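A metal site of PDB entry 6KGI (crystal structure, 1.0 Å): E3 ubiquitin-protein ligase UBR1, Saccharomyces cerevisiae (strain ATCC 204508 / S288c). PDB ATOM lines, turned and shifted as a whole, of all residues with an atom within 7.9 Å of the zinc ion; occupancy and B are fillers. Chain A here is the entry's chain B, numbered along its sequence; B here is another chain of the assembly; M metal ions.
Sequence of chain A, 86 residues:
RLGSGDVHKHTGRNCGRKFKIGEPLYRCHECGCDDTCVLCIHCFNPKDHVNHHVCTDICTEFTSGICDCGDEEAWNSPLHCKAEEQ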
ATOM      1  N   ARG A  27      -6.192 -30.847  -6.306  1.00  0.00           N
ATOM      2  CA  ARG A  27      -7.073 -29.762  -5.909  1.00  0.00           C
ATOM      3  C   ARG A  27      -6.751 -29.382  -4.469  1.00  0.00           C
ATOM      4  O   ARG A  27      -6.289 -30.211  -3.686  1.00  0.00           O
ATOM      5  CB  ARG A  27      -8.542 -30.201  -5.959  1.00  0.00           C
ATOM      6  CG  ARG A  27      -8.939 -30.858  -7.271  1.00  0.00           C
ATOM      7  CD  ARG A  27     -10.366 -31.459  -7.213  1.00  0.00           C
ATOM      8  NE  ARG A  27     -10.683 -32.167  -8.456  1.00  0.00           N
ATOM      9  CZ  ARG A  27     -11.102 -31.564  -9.570  1.00  0.00           C
ATOM     10  NH1 ARG A  27     -11.314 -30.257  -9.576  1.00  0.00           N
ATOM     11  NH2 ARG A  27     -11.318 -32.283 -10.663  1.00  0.00           N
ATOM     12  N   CYS A  28      -7.023 -28.122  -4.118  1.00  0.00           N
ATOM     13  CA  CYS A  28      -6.874 -27.661  -2.736  1.00  0.00           C
ATOM     14  C   CYS A  28      -8.134 -26.892  -2.340  1.00  0.00           C
ATOM     15  O   CYS A  28      -8.465 -25.884  -2.977  1.00  0.00           O
ATOM     16  CB  CYS A  28      -5.651 -26.775  -2.535  1.00  0.00           C
ATOM     17  SG  CYS A  28      -5.637 -26.161  -0.848  1.00  0.00           S
ATOM     18  N   HIS A  29      -8.819 -27.358  -1.306  1.00  0.00           N
ATOM     19  CA  HIS A  29     -10.061 -26.708  -0.912  1.00  0.00           C
ATOM     20  C   HIS A  29      -9.841 -25.237  -0.603  1.00  0.00           C
ATOM     21  O   HIS A  29     -10.619 -24.377  -1.030  1.00  0.00           O
ATOM     22  CB  HIS A  29     -10.657 -27.404   0.318  1.00  0.00           C
ATOM     23  CG  HIS A  29     -11.904 -26.762   0.826  1.00  0.00           C
ATOM     24  ND1 HIS A  29     -11.943 -25.998   1.973  1.00  0.00           N
ATOM     25  CD2 HIS A  29     -13.167 -26.755   0.329  1.00  0.00           C
ATOM     26  CE1 HIS A  29     -13.171 -25.558   2.173  1.00  0.00           C
ATOM     27  NE2 HIS A  29     -13.937 -25.997   1.185  1.00  0.00           N
ATOM     28  N   GLU A  30      -8.803 -24.920   0.176  1.00  0.00           N
ATOM     29  CA  GLU A  30      -8.594 -23.552   0.620  1.00  0.00           C
ATOM     30  C   GLU A  30      -8.074 -22.656  -0.499  1.00  0.00           C
ATOM     31  O   GLU A  30      -8.440 -21.474  -0.548  1.00  0.00           O
ATOM     32  CB  GLU A  30      -7.611 -23.532   1.784  1.00  0.00           C
ATOM     33  CG  GLU A  30      -8.175 -24.038   3.096  1.00  0.00           C
ATOM     34  CD  GLU A  30      -8.058 -25.552   3.286  1.00  0.00           C
ATOM     35  OE1 GLU A  30      -7.740 -26.293   2.331  1.00  0.00           O
ATOM     36  OE2 GLU A  30      -8.298 -26.007   4.428  1.00  0.00           O
ATOM     37  N   CYS A  31      -7.199 -23.172  -1.375  1.00  0.00           N
ATOM     38  CA  CYS A  31      -6.555 -22.291  -2.336  1.00  0.00           C
ATOM     39  C   CYS A  31      -7.403 -22.093  -3.585  1.00  0.00           C
ATOM     40  O   CYS A  31      -7.398 -20.996  -4.167  1.00  0.00           O
ATOM     41  CB  CYS A  31      -5.197 -22.853  -2.768  1.00  0.00           C
ATOM     42  SG  CYS A  31      -3.894 -22.713  -1.444  1.00  0.00           S
ATOM     43  N   GLY A  32      -8.100 -23.117  -4.054  1.00  0.00           N
ATOM     44  CA  GLY A  32      -8.859 -22.980  -5.292  1.00  0.00           C
ATOM     45  C   GLY A  32     -10.038 -22.042  -5.115  1.00  0.00           C
ATOM     46  O   GLY A  32     -10.798 -22.155  -4.150  1.00  0.00           O
ATOM     47  N   LEU A  39      -4.360 -28.248 -10.338  1.00  0.00           N
ATOM     48  CA  LEU A  39      -2.923 -28.186 -10.549  1.00  0.00           C
ATOM     49  C   LEU A  39      -2.405 -29.526 -11.031  1.00  0.00           C
ATOM     50  O   LEU A  39      -2.702 -30.580 -10.444  1.00  0.00           O
ATOM     51  CB  LEU A  39      -2.201 -27.822  -9.248  1.00  0.00           C
ATOM     52  CG  LEU A  39      -2.507 -26.427  -8.705  1.00  0.00           C
ATOM     53  CD1 LEU A  39      -2.083 -26.286  -7.253  1.00  0.00           C
ATOM     54  CD2 LEU A  39      -1.843 -25.364  -9.564  1.00  0.00           C
ATOM     55  N   PHE A  44       1.985 -28.707  -8.797  1.00  0.00           N
ATOM     56  CA  PHE A  44       1.546 -28.731  -7.415  1.00  0.00           C
ATOM     57  C   PHE A  44       2.749 -28.755  -6.482  1.00  0.00           C
ATOM     58  O   PHE A  44       3.607 -29.630  -6.589  1.00  0.00           O
ATOM     59  CB  PHE A  44       0.693 -29.975  -7.148  1.00  0.00           C
ATOM     60  CG  PHE A  44       0.259 -30.098  -5.706  1.00  0.00           C
ATOM     61  CD1 PHE A  44      -0.858 -29.420  -5.245  1.00  0.00           C
ATOM     62  CD2 PHE A  44       0.975 -30.877  -4.818  1.00  0.00           C
ATOM     63  CE1 PHE A  44      -1.251 -29.506  -3.910  1.00  0.00           C
ATOM     64  CE2 PHE A  44       0.586 -30.971  -3.488  1.00  0.00           C
ATOM     65  CZ  PHE A  44      -0.530 -30.285  -3.038  1.00  0.00           C
ATOM     66  N   ASN A  45       2.784 -27.799  -5.556  1.00  0.00           N
ATOM     67  CA  ASN A  45       3.900 -27.698  -4.631  1.00  0.00           C
ATOM     68  C   ASN A  45       3.390 -27.969  -3.230  1.00  0.00           C
ATOM     69  O   ASN A  45       2.627 -27.143  -2.688  1.00  0.00           O
ATOM     70  CB  ASN A  45       4.526 -26.310  -4.704  1.00  0.00           C
ATOM     71  CG  ASN A  45       5.809 -26.216  -3.912  1.00  0.00           C
ATOM     72  OD1 ASN A  45       6.069 -27.062  -3.052  1.00  0.00           O
ATOM     73  ND2 ASN A  45       6.620 -25.214  -4.204  1.00  0.00           N
ATOM     74  N   PRO A  46       3.753 -29.084  -2.602  1.00  0.00           N
ATOM     75  CA  PRO A  46       3.230 -29.356  -1.254  1.00  0.00           C
ATOM     76  C   PRO A  46       3.556 -28.267  -0.257  1.00  0.00           C
ATOM     77  O   PRO A  46       2.842 -28.118   0.747  1.00  0.00           O
ATOM     78  CB  PRO A  46       3.869 -30.711  -0.889  1.00  0.00           C
ATOM     79  CG  PRO A  46       5.077 -30.815  -1.773  1.00  0.00           C
ATOM     80  CD  PRO A  46       4.659 -30.154  -3.063  1.00  0.00           C
ATOM     81  N   LYS A  47       4.624 -27.494  -0.496  1.00  0.00           N
ATOM     82  CA  LYS A  47       4.984 -26.436   0.433  1.00  0.00           C
ATOM     83  C   LYS A  47       3.935 -25.331   0.479  1.00  0.00           C
ATOM     84  O   LYS A  47       3.939 -24.537   1.428  1.00  0.00           O
ATOM     85  CB  LYS A  47       6.315 -25.809   0.037  1.00  0.00           C
ATOM     86  CG  LYS A  47       7.512 -26.715   0.117  1.00  0.00           C
ATOM     87  CD  LYS A  47       8.746 -26.020  -0.433  1.00  0.00           C
ATOM     88  CE  LYS A  47       9.921 -26.957  -0.531  1.00  0.00           C
ATOM     89  NZ  LYS A  47      11.015 -26.351  -1.337  1.00  0.00           N
ATOM     90  N   ASP A  48       3.057 -25.227  -0.519  1.00  0.00           N
ATOM     91  CA  ASP A  48       2.045 -24.189  -0.540  1.00  0.00           C
ATOM     92  C   ASP A  48       0.806 -24.543   0.276  1.00  0.00           C
ATOM     93  O   ASP A  48      -0.071 -23.684   0.432  1.00  0.00           O
ATOM     94  CB  ASP A  48       1.568 -23.938  -1.979  1.00  0.00           C
ATOM     95  CG  ASP A  48       2.557 -23.141  -2.829  1.00  0.00           C
ATOM     96  OD1 ASP A  48       3.261 -22.270  -2.275  1.00  0.00           O
ATOM     97  OD2 ASP A  48       2.569 -23.364  -4.074  1.00  0.00           O
ATOM     98  N   HIS A  49       0.711 -25.760   0.783  1.00  0.00           N
ATOM     99  CA  HIS A  49      -0.577 -26.270   1.238  1.00  0.00           C
ATOM    100  C   HIS A  49      -0.541 -26.963   2.593  1.00  0.00           C
ATOM    101  O   HIS A  49      -1.430 -27.761   2.886  1.00  0.00           O
ATOM    102  CB  HIS A  49      -1.181 -27.205   0.187  1.00  0.00           C
ATOM    103  CG  HIS A  49      -1.221 -26.591  -1.170  1.00  0.00           C
ATOM    104  ND1 HIS A  49      -2.127 -25.613  -1.504  1.00  0.00           N
ATOM    105  CD2 HIS A  49      -0.449 -26.794  -2.265  1.00  0.00           C
ATOM    106  CE1 HIS A  49      -1.917 -25.237  -2.755  1.00  0.00           C
ATOM    107  NE2 HIS A  49      -0.893 -25.938  -3.243  1.00  0.00           N
ATOM    108  N   VAL A  50       0.429 -26.638   3.447  1.00  0.00           N
ATOM    109  CA  VAL A  50       0.510 -27.278   4.756  1.00  0.00           C
ATOM    110  C   VAL A  50      -0.780 -27.010   5.511  1.00  0.00           C
ATOM    111  O   VAL A  50      -1.219 -25.860   5.657  1.00  0.00           O
ATOM    112  CB  VAL A  50       1.751 -26.788   5.505  1.00  0.00           C
ATOM    113  CG1 VAL A  50       1.721 -27.288   6.949  1.00  0.00           C
ATOM    114  CG2 VAL A  50       3.007 -27.235   4.796  1.00  0.00           C
ATOM    115  N   ASN A  51      -1.395 -28.082   6.009  1.00  0.00           N
ATOM    116  CA  ASN A  51      -2.656 -28.028   6.758  1.00  0.00           C
ATOM    117  C   ASN A  51      -3.835 -27.554   5.919  1.00  0.00           C
ATOM    118  O   ASN A  51      -4.886 -27.207   6.471  1.00  0.00           O
ATOM    119  CB  ASN A  51      -2.540 -27.244   8.074  1.00  0.00           C
ATOM    120  CG  ASN A  51      -2.098 -28.129   9.221  1.00  0.00           C
ATOM    121  OD1 ASN A  51      -2.643 -29.231   9.412  1.00  0.00           O
ATOM    122  ND2 ASN A  51      -1.106 -27.678   9.975  1.00  0.00           N
ATOM    123  N   HIS A  52      -3.705 -27.554   4.591  1.00  0.00           N
ATOM    124  CA  HIS A  52      -4.863 -27.420   3.711  1.00  0.00           C
ATOM    125  C   HIS A  52      -5.440 -28.788   3.442  1.00  0.00           C
ATOM    126  O   HIS A  52      -4.793 -29.813   3.638  1.00  0.00           O
ATOM    127  CB  HIS A  52      -4.464 -26.758   2.401  1.00  0.00           C
ATOM    128  CG  HIS A  52      -4.287 -25.276   2.507  1.00  0.00           C
ATOM    129  ND1 HIS A  52      -3.823 -24.498   1.464  1.00  0.00           N
ATOM    130  CD2 HIS A  52      -4.564 -24.426   3.531  1.00  0.00           C
ATOM    131  CE1 HIS A  52      -3.824 -23.236   1.847  1.00  0.00           C
ATOM    132  NE2 HIS A  52      -4.254 -23.170   3.092  1.00  0.00           N
ATOM    133  N   HIS A  53      -6.694 -28.801   2.984  1.00  0.00           N
ATOM    134  CA  HIS A  53      -7.360 -30.040   2.595  1.00  0.00           C
ATOM    135  C   HIS A  53      -7.127 -30.250   1.109  1.00  0.00           C
ATOM    136  O   HIS A  53      -7.801 -29.656   0.262  1.00  0.00           O
ATOM    137  CB  HIS A  53      -8.839 -30.005   2.946  1.00  0.00           C
ATOM    138  CG  HIS A  53      -9.567 -31.269   2.645  1.00  0.00           C
ATOM    139  ND1 HIS A  53     -10.723 -31.633   3.300  1.00  0.00           N
ATOM    140  CD2 HIS A  53      -9.304 -32.273   1.771  1.00  0.00           C
ATOM    141  CE1 HIS A  53     -11.158 -32.795   2.827  1.00  0.00           C
ATOM    142  NE2 HIS A  53     -10.310 -33.200   1.894  1.00  0.00           N
ATOM    143  N   VAL A  54      -6.141 -31.081   0.795  1.00  0.00           N
ATOM    144  CA  VAL A  54      -5.791 -31.394  -0.585  1.00  0.00           C
ATOM    145  C   VAL A  54      -6.538 -32.652  -0.996  1.00  0.00           C
ATOM    146  O   VAL A  54      -6.736 -33.584  -0.202  1.00  0.00           O
ATOM    147  CB  VAL A  54      -4.264 -31.545  -0.709  1.00  0.00           C
ATOM    148  CG1 VAL A  54      -3.865 -32.222  -2.006  1.00  0.00           C
ATOM    149  CG2 VAL A  54      -3.606 -30.165  -0.594  1.00  0.00           C
ATOM    150  N   TRP A  75      -6.846 -18.827  -7.845  1.00  0.00           N
ATOM    151  CA  TRP A  75      -6.242 -19.133  -6.559  1.00  0.00           C
ATOM    152  C   TRP A  75      -6.413 -17.967  -5.589  1.00  0.00           C
ATOM    153  O   TRP A  75      -6.396 -16.803  -5.978  1.00  0.00           O
ATOM    154  CB  TRP A  75      -4.743 -19.485  -6.719  1.00  0.00           C
ATOM    155  CG  TRP A  75      -4.572 -20.551  -7.766  1.00  0.00           C
ATOM    156  CD1 TRP A  75      -4.055 -20.409  -9.015  1.00  0.00           C
ATOM    157  CD2 TRP A  75      -4.976 -21.920  -7.647  1.00  0.00           C
ATOM    158  NE1 TRP A  75      -4.098 -21.624  -9.680  1.00  0.00           N
ATOM    159  CE2 TRP A  75      -4.667 -22.558  -8.859  1.00  0.00           C
ATOM    160  CE3 TRP A  75      -5.563 -22.666  -6.622  1.00  0.00           C
ATOM    161  CZ2 TRP A  75      -4.928 -23.913  -9.076  1.00  0.00           C
ATOM    162  CZ3 TRP A  75      -5.831 -23.998  -6.841  1.00  0.00           C
ATOM    163  CH2 TRP A  75      -5.510 -24.601  -8.054  1.00  0.00           C
ATOM    164  N   SER A  77      -4.365 -17.475  -2.883  1.00  0.00           N
ATOM    165  CA  SER A  77      -3.063 -17.134  -2.323  1.00  0.00           C
ATOM    166  C   SER A  77      -2.047 -17.288  -3.444  1.00  0.00           C
ATOM    167  O   SER A  77      -2.283 -18.036  -4.404  1.00  0.00           O
ATOM    168  CB  SER A  77      -2.634 -18.113  -1.225  1.00  0.00           C
ATOM    169  OG  SER A  77      -3.726 -18.524  -0.415  1.00  0.00           O
ATOM    170  N   PRO A  78      -0.875 -16.660  -3.315  1.00  0.00           N
ATOM    171  CA  PRO A  78       0.198 -16.963  -4.272  1.00  0.00           C
ATOM    172  C   PRO A  78       0.620 -18.412  -4.185  1.00  0.00           C
ATOM    173  O   PRO A  78       0.771 -18.967  -3.094  1.00  0.00           O
ATOM    174  CB  PRO A  78       1.331 -16.020  -3.845  1.00  0.00           C
ATOM    175  CG  PRO A  78       0.676 -14.930  -3.085  1.00  0.00           C
ATOM    176  CD  PRO A  78      -0.498 -15.576  -2.392  1.00  0.00           C
ATOM    177  N   LEU A  79       0.817 -19.024  -5.349  1.00  0.00           N
ATOM    178  CA  LEU A  79       1.431 -20.338  -5.432  1.00  0.00           C
ATOM    179  C   LEU A  79       2.880 -20.187  -5.857  1.00  0.00           C
ATOM    180  O   LEU A  79       3.293 -19.153  -6.393  1.00  0.00           O
ATOM    181  CB  LEU A  79       0.700 -21.207  -6.453  1.00  0.00           C
ATOM    182  CG  LEU A  79      -0.784 -21.427  -6.156  1.00  0.00           C
ATOM    183  CD1 LEU A  79      -1.370 -22.366  -7.209  1.00  0.00           C
ATOM    184  CD2 LEU A  79      -1.005 -21.972  -4.747  1.00  0.00           C
ATOM    185  N   THR B  56      -0.335 -31.937   3.580  1.00  0.00           N
ATOM    186  CA  THR B  56       1.113 -31.828   3.471  1.00  0.00           C
ATOM    187  C   THR B  56       1.692 -31.232   4.752  1.00  0.00           C
ATOM    188  O   THR B  56       0.987 -30.682   5.602  1.00  0.00           O
ATOM    189  CB  THR B  56       1.507 -30.992   2.254  1.00  0.00           C
ATOM    190  OG1 THR B  56       1.170 -29.630   2.487  1.00  0.00           O
ATOM    191  CG2 THR B  56       0.826 -31.511   0.988  1.00  0.00           C
HETATM  192 ZN    ZN M   1      -3.808 -24.828  -0.568  1.00  0.00          ZN
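The backbone NH (N) of Glu 30 lies close to the side-chain sulfur (SG) of Cys 28 (3.6 Å).
O of His 49 lies close to OG1 of Thr 56 of chain B (3.2 Å).
Within 4 Å of the zinc ion: Cys 28, Cys 31, His 49 and His 52.
ND1 of His 52 binds the zinc ion.
ND1 of His 49 binds the zinc ion, 2.1 Å away.
The zinc ion is bound by SG of Cys 28 (2.3 Å).
The zinc ion is bound by the side-chain sulfur (SG) of Cys 31, at 2.3 Å.
The zinc ion has four donor atoms within binding distance.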
